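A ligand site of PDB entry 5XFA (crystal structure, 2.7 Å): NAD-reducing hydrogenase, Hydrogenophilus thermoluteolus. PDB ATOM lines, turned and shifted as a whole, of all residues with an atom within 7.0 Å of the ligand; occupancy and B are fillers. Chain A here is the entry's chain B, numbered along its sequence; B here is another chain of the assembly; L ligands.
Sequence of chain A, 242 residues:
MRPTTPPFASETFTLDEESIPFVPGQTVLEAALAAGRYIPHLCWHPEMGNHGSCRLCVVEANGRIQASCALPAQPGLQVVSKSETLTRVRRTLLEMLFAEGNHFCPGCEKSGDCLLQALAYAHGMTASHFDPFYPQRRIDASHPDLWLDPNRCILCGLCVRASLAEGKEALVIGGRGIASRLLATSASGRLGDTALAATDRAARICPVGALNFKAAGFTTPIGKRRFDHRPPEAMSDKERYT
Phe 98 touches the ligand (CZ to S2, 3.8 Å).
Phe 104 touches the ligand.
Lys 110 touches the ligand.
CD2 of Leu 116 touches S2 of the ligand (3.6 Å).
Val 208 touches the ligand.
Hydrophobic or aromatic side chains within 4 Å of the ligand: Phe 98, His 103, Leu 116 and Val 208.
Within 4 Å of the ligand: Phe 98, His 103, Phe 104, Cys 105, Cys 108, Lys 110, Ser 111, Cys 114, Leu 116, Gln 117, Val 208 and Gly 209.
The backbone carbonyl oxygen (O) of Val 208 sits at hydrogen-bond distance from the side-chain amino group (NZ) of Lys 110 (3.1 Å).
SG of Cys 114 lies close to N of Leu 116.
The side-chain sulfur (SG) of Cys 105 lies close to the side-chain amide nitrogen (NE2) of Gln 117 (3.1 Å).
The backbone NH (N) of Gly 112 is in hydrogen-bond range of the side-chain amide oxygen (OE1) of Gln 117.
The side-chain amide nitrogen (NE2) of Gln 117 sits at hydrogen-bond distance from the side-chain hydroxyl (OG) of Ser 111, 3.0 Å away.
The side-chain sulfur (SG) of Cys 108 sits close to the backbone NH (N) of Lys 110 (3.3 Å).
SG of Cys 114 lies close to N of Gln 117 (3.5 Å).
A sulfur (S3) of the ligand sits close to the backbone NH (N) of Cys 105, 3.5 Å away.
SG of Cys 105 is bound to FE1 of the ligand.
SG of Cys 114 is bound to FE3 of the ligand (2.3 Å).
A sulfur (S1) of the ligand lies close to the backbone NH (N) of Gly 209 (3.0 Å).
The backbone NH (N) of Ser 111 lies close to a sulfur (S4) of the ligand, at 3.8 Å.
S4 of the ligand sits close to NE2 of Gln 117, 3.4 Å away.
SG of Cys 108 is bound to FE2 of the ligand, 2.3 Å away.
A ring nitrogen (ND1) of His 103 is bound to an iron atom (FE4) of the ligand.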
ATOM      1  N   PHE A  98     -11.422  25.081   4.332  1.00  0.00           N
ATOM      2  CA  PHE A  98     -10.469  24.056   4.729  1.00  0.00           C
ATOM      3  C   PHE A  98      -9.880  24.357   6.104  1.00  0.00           C
ATOM      4  O   PHE A  98      -9.865  23.478   6.982  1.00  0.00           O
ATOM      5  CB  PHE A  98      -9.381  23.936   3.695  1.00  0.00           C
ATOM      6  CG  PHE A  98      -9.704  22.978   2.581  1.00  0.00           C
ATOM      7  CD1 PHE A  98     -10.375  23.395   1.448  1.00  0.00           C
ATOM      8  CD2 PHE A  98      -9.326  21.658   2.650  1.00  0.00           C
ATOM      9  CE1 PHE A  98     -10.685  22.524   0.409  1.00  0.00           C
ATOM     10  CE2 PHE A  98      -9.614  20.786   1.607  1.00  0.00           C
ATOM     11  CZ  PHE A  98     -10.299  21.219   0.493  1.00  0.00           C
ATOM     12  N   ASN A 102     -11.907  20.101   9.858  1.00  0.00           N
ATOM     13  CA  ASN A 102     -10.880  19.085   9.818  1.00  0.00           C
ATOM     14  C   ASN A 102     -11.042  18.337   8.495  1.00  0.00           C
ATOM     15  O   ASN A 102     -11.709  17.297   8.419  1.00  0.00           O
ATOM     16  CB  ASN A 102     -11.011  18.127  10.999  1.00  0.00           C
ATOM     17  CG  ASN A 102     -10.922  18.827  12.342  1.00  0.00           C
ATOM     18  OD1 ASN A 102     -10.153  19.783  12.524  1.00  0.00           O
ATOM     19  ND2 ASN A 102     -11.731  18.379  13.304  1.00  0.00           N
ATOM     20  N   HIS A 103     -10.455  18.921   7.453  1.00  0.00           N
ATOM     21  CA  HIS A 103     -10.382  18.287   6.153  1.00  0.00           C
ATOM     22  C   HIS A 103      -9.015  17.640   5.934  1.00  0.00           C
ATOM     23  O   HIS A 103      -8.152  18.082   5.136  1.00  0.00           O
ATOM     24  CB  HIS A 103     -10.747  19.279   5.066  1.00  0.00           C
ATOM     25  CG  HIS A 103     -12.042  19.934   5.312  1.00  0.00           C
ATOM     26  ND1 HIS A 103     -13.234  19.389   4.897  1.00  0.00           N
ATOM     27  CD2 HIS A 103     -12.355  21.022   6.040  1.00  0.00           C
ATOM     28  CE1 HIS A 103     -14.221  20.148   5.317  1.00  0.00           C
ATOM     29  NE2 HIS A 103     -13.712  21.151   5.994  1.00  0.00           N
ATOM     30  N   PHE A 104      -8.888  16.568   6.686  1.00  0.00           N
ATOM     31  CA  PHE A 104      -8.010  15.490   6.460  1.00  0.00           C
ATOM     32  C   PHE A 104      -8.596  14.575   5.392  1.00  0.00           C
ATOM     33  O   PHE A 104      -8.988  13.453   5.689  1.00  0.00           O
ATOM     34  CB  PHE A 104      -7.921  14.723   7.791  1.00  0.00           C
ATOM     35  CG  PHE A 104      -7.594  15.606   8.962  1.00  0.00           C
ATOM     36  CD1 PHE A 104      -6.671  16.633   8.833  1.00  0.00           C
ATOM     37  CD2 PHE A 104      -8.189  15.420  10.169  1.00  0.00           C
ATOM     38  CE1 PHE A 104      -6.347  17.468   9.892  1.00  0.00           C
ATOM     39  CE2 PHE A 104      -7.868  16.250  11.241  1.00  0.00           C
ATOM     40  CZ  PHE A 104      -6.951  17.286  11.099  1.00  0.00           C
ATOM     41  N   CYS A 105      -8.613  15.018   4.137  1.00  0.00           N
ATOM     42  CA  CYS A 105      -9.055  14.134   3.042  1.00  0.00           C
ATOM     43  C   CYS A 105      -8.454  12.702   3.054  1.00  0.00           C
ATOM     44  O   CYS A 105      -9.136  11.777   2.641  1.00  0.00           O
ATOM     45  CB  CYS A 105      -8.741  14.763   1.682  1.00  0.00           C
ATOM     46  SG  CYS A 105      -9.275  16.482   1.516  1.00  0.00           S
ATOM     47  N   PRO A 106      -7.178  12.508   3.513  1.00  0.00           N
ATOM     48  CA  PRO A 106      -6.592  11.150   3.427  1.00  0.00           C
ATOM     49  C   PRO A 106      -7.336   9.992   4.115  1.00  0.00           C
ATOM     50  O   PRO A 106      -7.040   8.835   3.844  1.00  0.00           O
ATOM     51  CB  PRO A 106      -5.220  11.317   4.098  1.00  0.00           C
ATOM     52  CG  PRO A 106      -4.868  12.738   3.867  1.00  0.00           C
ATOM     53  CD  PRO A 106      -6.175  13.475   3.980  1.00  0.00           C
ATOM     54  N   GLY A 107      -8.256  10.315   5.016  1.00  0.00           N
ATOM     55  CA  GLY A 107      -9.064   9.289   5.617  1.00  0.00           C
ATOM     56  C   GLY A 107     -10.541   9.574   5.552  1.00  0.00           C
ATOM     57  O   GLY A 107     -11.306   8.997   6.334  1.00  0.00           O
ATOM     58  N   CYS A 108     -10.919  10.500   4.629  1.00  0.00           N
ATOM     59  CA  CYS A 108     -12.315  10.888   4.373  1.00  0.00           C
ATOM     60  C   CYS A 108     -12.826  10.006   3.279  1.00  0.00           C
ATOM     61  O   CYS A 108     -12.173   9.841   2.236  1.00  0.00           O
ATOM     62  CB  CYS A 108     -12.426  12.318   3.893  1.00  0.00           C
ATOM     63  SG  CYS A 108     -14.120  12.893   3.522  1.00  0.00           S
ATOM     64  N   GLU A 109     -14.016   9.466   3.507  1.00  0.00           N
ATOM     65  CA  GLU A 109     -14.593   8.526   2.585  1.00  0.00           C
ATOM     66  C   GLU A 109     -15.254   9.271   1.402  1.00  0.00           C
ATOM     67  O   GLU A 109     -15.709   8.613   0.468  1.00  0.00           O
ATOM     68  CB  GLU A 109     -15.569   7.630   3.324  1.00  0.00           C
ATOM     69  CG  GLU A 109     -16.962   8.252   3.514  1.00  0.00           C
ATOM     70  CD  GLU A 109     -17.796   7.510   4.527  1.00  0.00           C
ATOM     71  OE1 GLU A 109     -17.525   7.692   5.734  1.00  0.00           O
ATOM     72  OE2 GLU A 109     -18.700   6.745   4.112  1.00  0.00           O
ATOM     73  N   LYS A 110     -15.291  10.609   1.412  1.00  0.00           N
ATOM     74  CA  LYS A 110     -15.645  11.331   0.201  1.00  0.00           C
ATOM     75  C   LYS A 110     -14.468  11.888  -0.610  1.00  0.00           C
ATOM     76  O   LYS A 110     -14.673  12.589  -1.574  1.00  0.00           O
ATOM     77  CB  LYS A 110     -16.657  12.477   0.439  1.00  0.00           C
ATOM     78  CG  LYS A 110     -17.991  12.132   1.089  1.00  0.00           C
ATOM     79  CD  LYS A 110     -18.758  10.993   0.422  1.00  0.00           C
ATOM     80  CE  LYS A 110     -20.284  11.044   0.704  1.00  0.00           C
ATOM     81  NZ  LYS A 110     -20.979  12.349   0.484  1.00  0.00           N
ATOM     82  N   SER A 111     -13.241  11.482  -0.327  1.00  0.00           N
ATOM     83  CA  SER A 111     -12.119  11.959  -1.164  1.00  0.00           C
ATOM     84  C   SER A 111     -12.335  11.505  -2.611  1.00  0.00           C
ATOM     85  O   SER A 111     -12.637  10.340  -2.874  1.00  0.00           O
ATOM     86  CB  SER A 111     -10.769  11.486  -0.634  1.00  0.00           C
ATOM     87  OG  SER A 111      -9.741  12.395  -0.979  1.00  0.00           O
ATOM     88  N   GLY A 112     -12.245  12.450  -3.543  1.00  0.00           N
ATOM     89  CA  GLY A 112     -12.466  12.175  -4.953  1.00  0.00           C
ATOM     90  C   GLY A 112     -13.926  12.179  -5.323  1.00  0.00           C
ATOM     91  O   GLY A 112     -14.259  12.051  -6.515  1.00  0.00           O
ATOM     92  N   ASP A 113     -14.810  12.318  -4.323  1.00  0.00           N
ATOM     93  CA  ASP A 113     -16.250  12.296  -4.537  1.00  0.00           C
ATOM     94  C   ASP A 113     -16.839  13.505  -3.798  1.00  0.00           C
ATOM     95  O   ASP A 113     -17.957  13.488  -3.409  1.00  0.00           O
ATOM     96  CB  ASP A 113     -16.801  10.951  -4.025  1.00  0.00           C
ATOM     97  CG  ASP A 113     -18.327  10.816  -4.131  1.00  0.00           C
ATOM     98  OD1 ASP A 113     -18.860  10.636  -5.247  1.00  0.00           O
ATOM     99  OD2 ASP A 113     -18.997  10.866  -3.066  1.00  0.00           O
ATOM    100  N   CYS A 114     -16.045  14.567  -3.679  1.00  0.00           N
ATOM    101  CA  CYS A 114     -16.327  15.711  -2.815  1.00  0.00           C
ATOM    102  C   CYS A 114     -16.117  17.019  -3.582  1.00  0.00           C
ATOM    103  O   CYS A 114     -15.046  17.240  -4.151  1.00  0.00           O
ATOM    104  CB  CYS A 114     -15.377  15.674  -1.640  1.00  0.00           C
ATOM    105  SG  CYS A 114     -15.303  17.172  -0.642  1.00  0.00           S
ATOM    106  N   LEU A 115     -17.111  17.908  -3.538  1.00  0.00           N
ATOM    107  CA  LEU A 115     -17.163  19.115  -4.361  1.00  0.00           C
ATOM    108  C   LEU A 115     -16.198  20.157  -3.859  1.00  0.00           C
ATOM    109  O   LEU A 115     -15.559  20.856  -4.660  1.00  0.00           O
ATOM    110  CB  LEU A 115     -18.586  19.703  -4.369  1.00  0.00           C
ATOM    111  CG  LEU A 115     -18.993  20.784  -5.393  1.00  0.00           C
ATOM    112  CD1 LEU A 115     -18.691  20.377  -6.835  1.00  0.00           C
ATOM    113  CD2 LEU A 115     -20.488  21.057  -5.290  1.00  0.00           C
ATOM    114  N   LEU A 116     -16.115  20.308  -2.541  1.00  0.00           N
ATOM    115  CA  LEU A 116     -15.199  21.241  -1.928  1.00  0.00           C
ATOM    116  C   LEU A 116     -13.792  20.913  -2.372  1.00  0.00           C
ATOM    117  O   LEU A 116     -13.054  21.791  -2.844  1.00  0.00           O
ATOM    118  CB  LEU A 116     -15.298  21.168  -0.402  1.00  0.00           C
ATOM    119  CG  LEU A 116     -14.171  21.822   0.396  1.00  0.00           C
ATOM    120  CD1 LEU A 116     -14.016  23.278   0.028  1.00  0.00           C
ATOM    121  CD2 LEU A 116     -14.397  21.684   1.892  1.00  0.00           C
ATOM    122  N   GLN A 117     -13.408  19.645  -2.235  1.00  0.00           N
ATOM    123  CA  GLN A 117     -12.098  19.204  -2.643  1.00  0.00           C
ATOM    124  C   GLN A 117     -11.934  19.476  -4.109  1.00  0.00           C
ATOM    125  O   GLN A 117     -10.944  20.067  -4.499  1.00  0.00           O
ATOM    126  CB  GLN A 117     -11.917  17.713  -2.348  1.00  0.00           C
ATOM    127  CG  GLN A 117     -10.652  17.086  -2.899  1.00  0.00           C
ATOM    128  CD  GLN A 117     -10.531  15.632  -2.487  1.00  0.00           C
ATOM    129  OE1 GLN A 117     -10.789  14.711  -3.272  1.00  0.00           O
ATOM    130  NE2 GLN A 117     -10.145  15.401  -1.236  1.00  0.00           N
ATOM    131  N   ALA A 118     -12.906  19.103  -4.936  1.00  0.00           N
ATOM    132  CA  ALA A 118     -12.715  19.260  -6.379  1.00  0.00           C
ATOM    133  C   ALA A 118     -12.569  20.743  -6.754  1.00  0.00           C
ATOM    134  O   ALA A 118     -11.763  21.083  -7.603  1.00  0.00           O
ATOM    135  CB  ALA A 118     -13.837  18.615  -7.181  1.00  0.00           C
ATOM    136  N   ASN A 151     -17.314  18.097  11.663  1.00  0.00           N
ATOM    137  CA  ASN A 151     -16.064  18.850  11.491  1.00  0.00           C
ATOM    138  C   ASN A 151     -15.647  19.001  10.040  1.00  0.00           C
ATOM    139  O   ASN A 151     -14.677  19.701   9.734  1.00  0.00           O
ATOM    140  CB  ASN A 151     -14.950  18.199  12.320  1.00  0.00           C
ATOM    141  CG  ASN A 151     -15.196  18.314  13.809  1.00  0.00           C
ATOM    142  OD1 ASN A 151     -15.297  19.433  14.346  1.00  0.00           O
ATOM    143  ND2 ASN A 151     -15.365  17.183  14.475  1.00  0.00           N
ATOM    144  N   ARG A 152     -16.393  18.334   9.164  1.00  0.00           N
ATOM    145  CA  ARG A 152     -16.285  18.465   7.724  1.00  0.00           C
ATOM    146  C   ARG A 152     -17.396  19.369   7.108  1.00  0.00           C
ATOM    147  O   ARG A 152     -17.293  19.761   5.945  1.00  0.00           O
ATOM    148  CB  ARG A 152     -16.376  17.060   7.106  1.00  0.00           C
ATOM    149  CG  ARG A 152     -15.151  16.197   7.406  1.00  0.00           C
ATOM    150  CD  ARG A 152     -15.386  14.760   7.031  1.00  0.00           C
ATOM    151  NE  ARG A 152     -14.226  13.924   7.313  1.00  0.00           N
ATOM    152  CZ  ARG A 152     -14.256  12.589   7.282  1.00  0.00           C
ATOM    153  NH1 ARG A 152     -15.392  11.941   6.978  1.00  0.00           N
ATOM    154  NH2 ARG A 152     -13.173  11.882   7.535  1.00  0.00           N
ATOM    155  N   CYS A 153     -18.449  19.657   7.874  1.00  0.00           N
ATOM    156  CA  CYS A 153     -19.618  20.331   7.359  1.00  0.00           C
ATOM    157  C   CYS A 153     -19.390  21.796   7.018  1.00  0.00           C
ATOM    158  O   CYS A 153     -18.825  22.550   7.813  1.00  0.00           O
ATOM    159  CB  CYS A 153     -20.668  20.273   8.426  1.00  0.00           C
ATOM    160  SG  CYS A 153     -22.158  21.195   8.123  1.00  0.00           S
ATOM    161  N   ILE A 154     -19.815  22.204   5.842  1.00  0.00           N
ATOM    162  CA  ILE A 154     -19.493  23.549   5.352  1.00  0.00           C
ATOM    163  C   ILE A 154     -20.693  24.478   5.421  1.00  0.00           C
ATOM    164  O   ILE A 154     -20.653  25.562   4.849  1.00  0.00           O
ATOM    165  CB  ILE A 154     -19.037  23.504   3.896  1.00  0.00           C
ATOM    166  CG1 ILE A 154     -20.151  22.936   3.002  1.00  0.00           C
ATOM    167  CG2 ILE A 154     -17.739  22.711   3.783  1.00  0.00           C
ATOM    168  CD1 ILE A 154     -19.932  23.143   1.515  1.00  0.00           C
ATOM    169  N   PRO A 207     -22.793  17.538  -0.232  1.00  0.00           N
ATOM    170  CA  PRO A 207     -21.790  17.573  -1.272  1.00  0.00           C
ATOM    171  C   PRO A 207     -20.336  17.329  -0.786  1.00  0.00           C
ATOM    172  O   PRO A 207     -19.421  17.248  -1.619  1.00  0.00           O
ATOM    173  CB  PRO A 207     -21.940  18.995  -1.817  1.00  0.00           C
ATOM    174  CG  PRO A 207     -22.231  19.792  -0.617  1.00  0.00           C
ATOM    175  CD  PRO A 207     -23.091  18.900   0.248  1.00  0.00           C
ATOM    176  N   VAL A 208     -20.148  17.258   0.523  1.00  0.00           N
ATOM    177  CA  VAL A 208     -18.848  16.944   1.126  1.00  0.00           C
ATOM    178  C   VAL A 208     -18.997  15.684   1.995  1.00  0.00           C
ATOM    179  O   VAL A 208     -19.947  14.959   1.832  1.00  0.00           O
ATOM    180  CB  VAL A 208     -18.249  18.151   1.877  1.00  0.00           C
ATOM    181  CG1 VAL A 208     -18.209  19.359   0.951  1.00  0.00           C
ATOM    182  CG2 VAL A 208     -19.045  18.491   3.135  1.00  0.00           C
ATOM    183  N   GLY A 209     -18.049  15.396   2.881  1.00  0.00           N
ATOM    184  CA  GLY A 209     -18.059  14.180   3.718  1.00  0.00           C
ATOM    185  C   GLY A 209     -18.720  14.331   5.102  1.00  0.00           C
ATOM    186  O   GLY A 209     -18.471  13.521   5.987  1.00  0.00           O
ATOM    187  N   ALA A 210     -19.597  15.307   5.266  1.00  0.00           N
ATOM    188  CA  ALA A 210     -20.274  15.550   6.534  1.00  0.00           C
ATOM    189  C   ALA A 210     -21.339  14.516   6.800  1.00  0.00           C
ATOM    190  O   ALA A 210     -21.177  13.694   7.717  1.00  0.00           O
ATOM    191  CB  ALA A 210     -20.910  16.921   6.561  1.00  0.00           C
ATOM    192  N   TYR B 188      -4.850  15.571  -2.424  1.00  0.00           N
ATOM    193  CA  TYR B 188      -4.729  15.772  -1.001  1.00  0.00           C
ATOM    194  C   TYR B 188      -4.877  14.431  -0.288  1.00  0.00           C
ATOM    195  O   TYR B 188      -4.925  14.387   0.928  1.00  0.00           O
ATOM    196  CB  TYR B 188      -5.865  16.694  -0.512  1.00  0.00           C
ATOM    197  CG  TYR B 188      -5.997  18.023  -1.189  1.00  0.00           C
ATOM    198  CD1 TYR B 188      -4.948  18.617  -1.882  1.00  0.00           C
ATOM    199  CD2 TYR B 188      -7.203  18.736  -1.088  1.00  0.00           C
ATOM    200  CE1 TYR B 188      -5.108  19.855  -2.469  1.00  0.00           C
ATOM    201  CE2 TYR B 188      -7.368  19.966  -1.672  1.00  0.00           C
ATOM    202  CZ  TYR B 188      -6.318  20.519  -2.371  1.00  0.00           C
ATOM    203  OH  TYR B 188      -6.524  21.736  -2.953  1.00  0.00           O
HETATM  204 FE1  LIG L   1     -11.522  16.553   2.077  1.00  0.00          FE
HETATM  205 FE2  LIG L   1     -13.261  15.002   3.206  1.00  0.00          FE
HETATM  206 FE3  LIG L   1     -14.111  16.830   1.247  1.00  0.00          FE
HETATM  207 FE4  LIG L   1     -13.582  17.706   3.585  1.00  0.00          FE
HETATM  208  S1  LIG L   1     -15.179  16.223   3.096  1.00  0.00           S
HETATM  209  S2  LIG L   1     -12.673  18.500   1.713  1.00  0.00           S
HETATM  210  S3  LIG L   1     -11.825  16.339   4.269  1.00  0.00           S
HETATM  211  S4  LIG L   1     -12.701  14.958   1.032  1.00  0.00           S
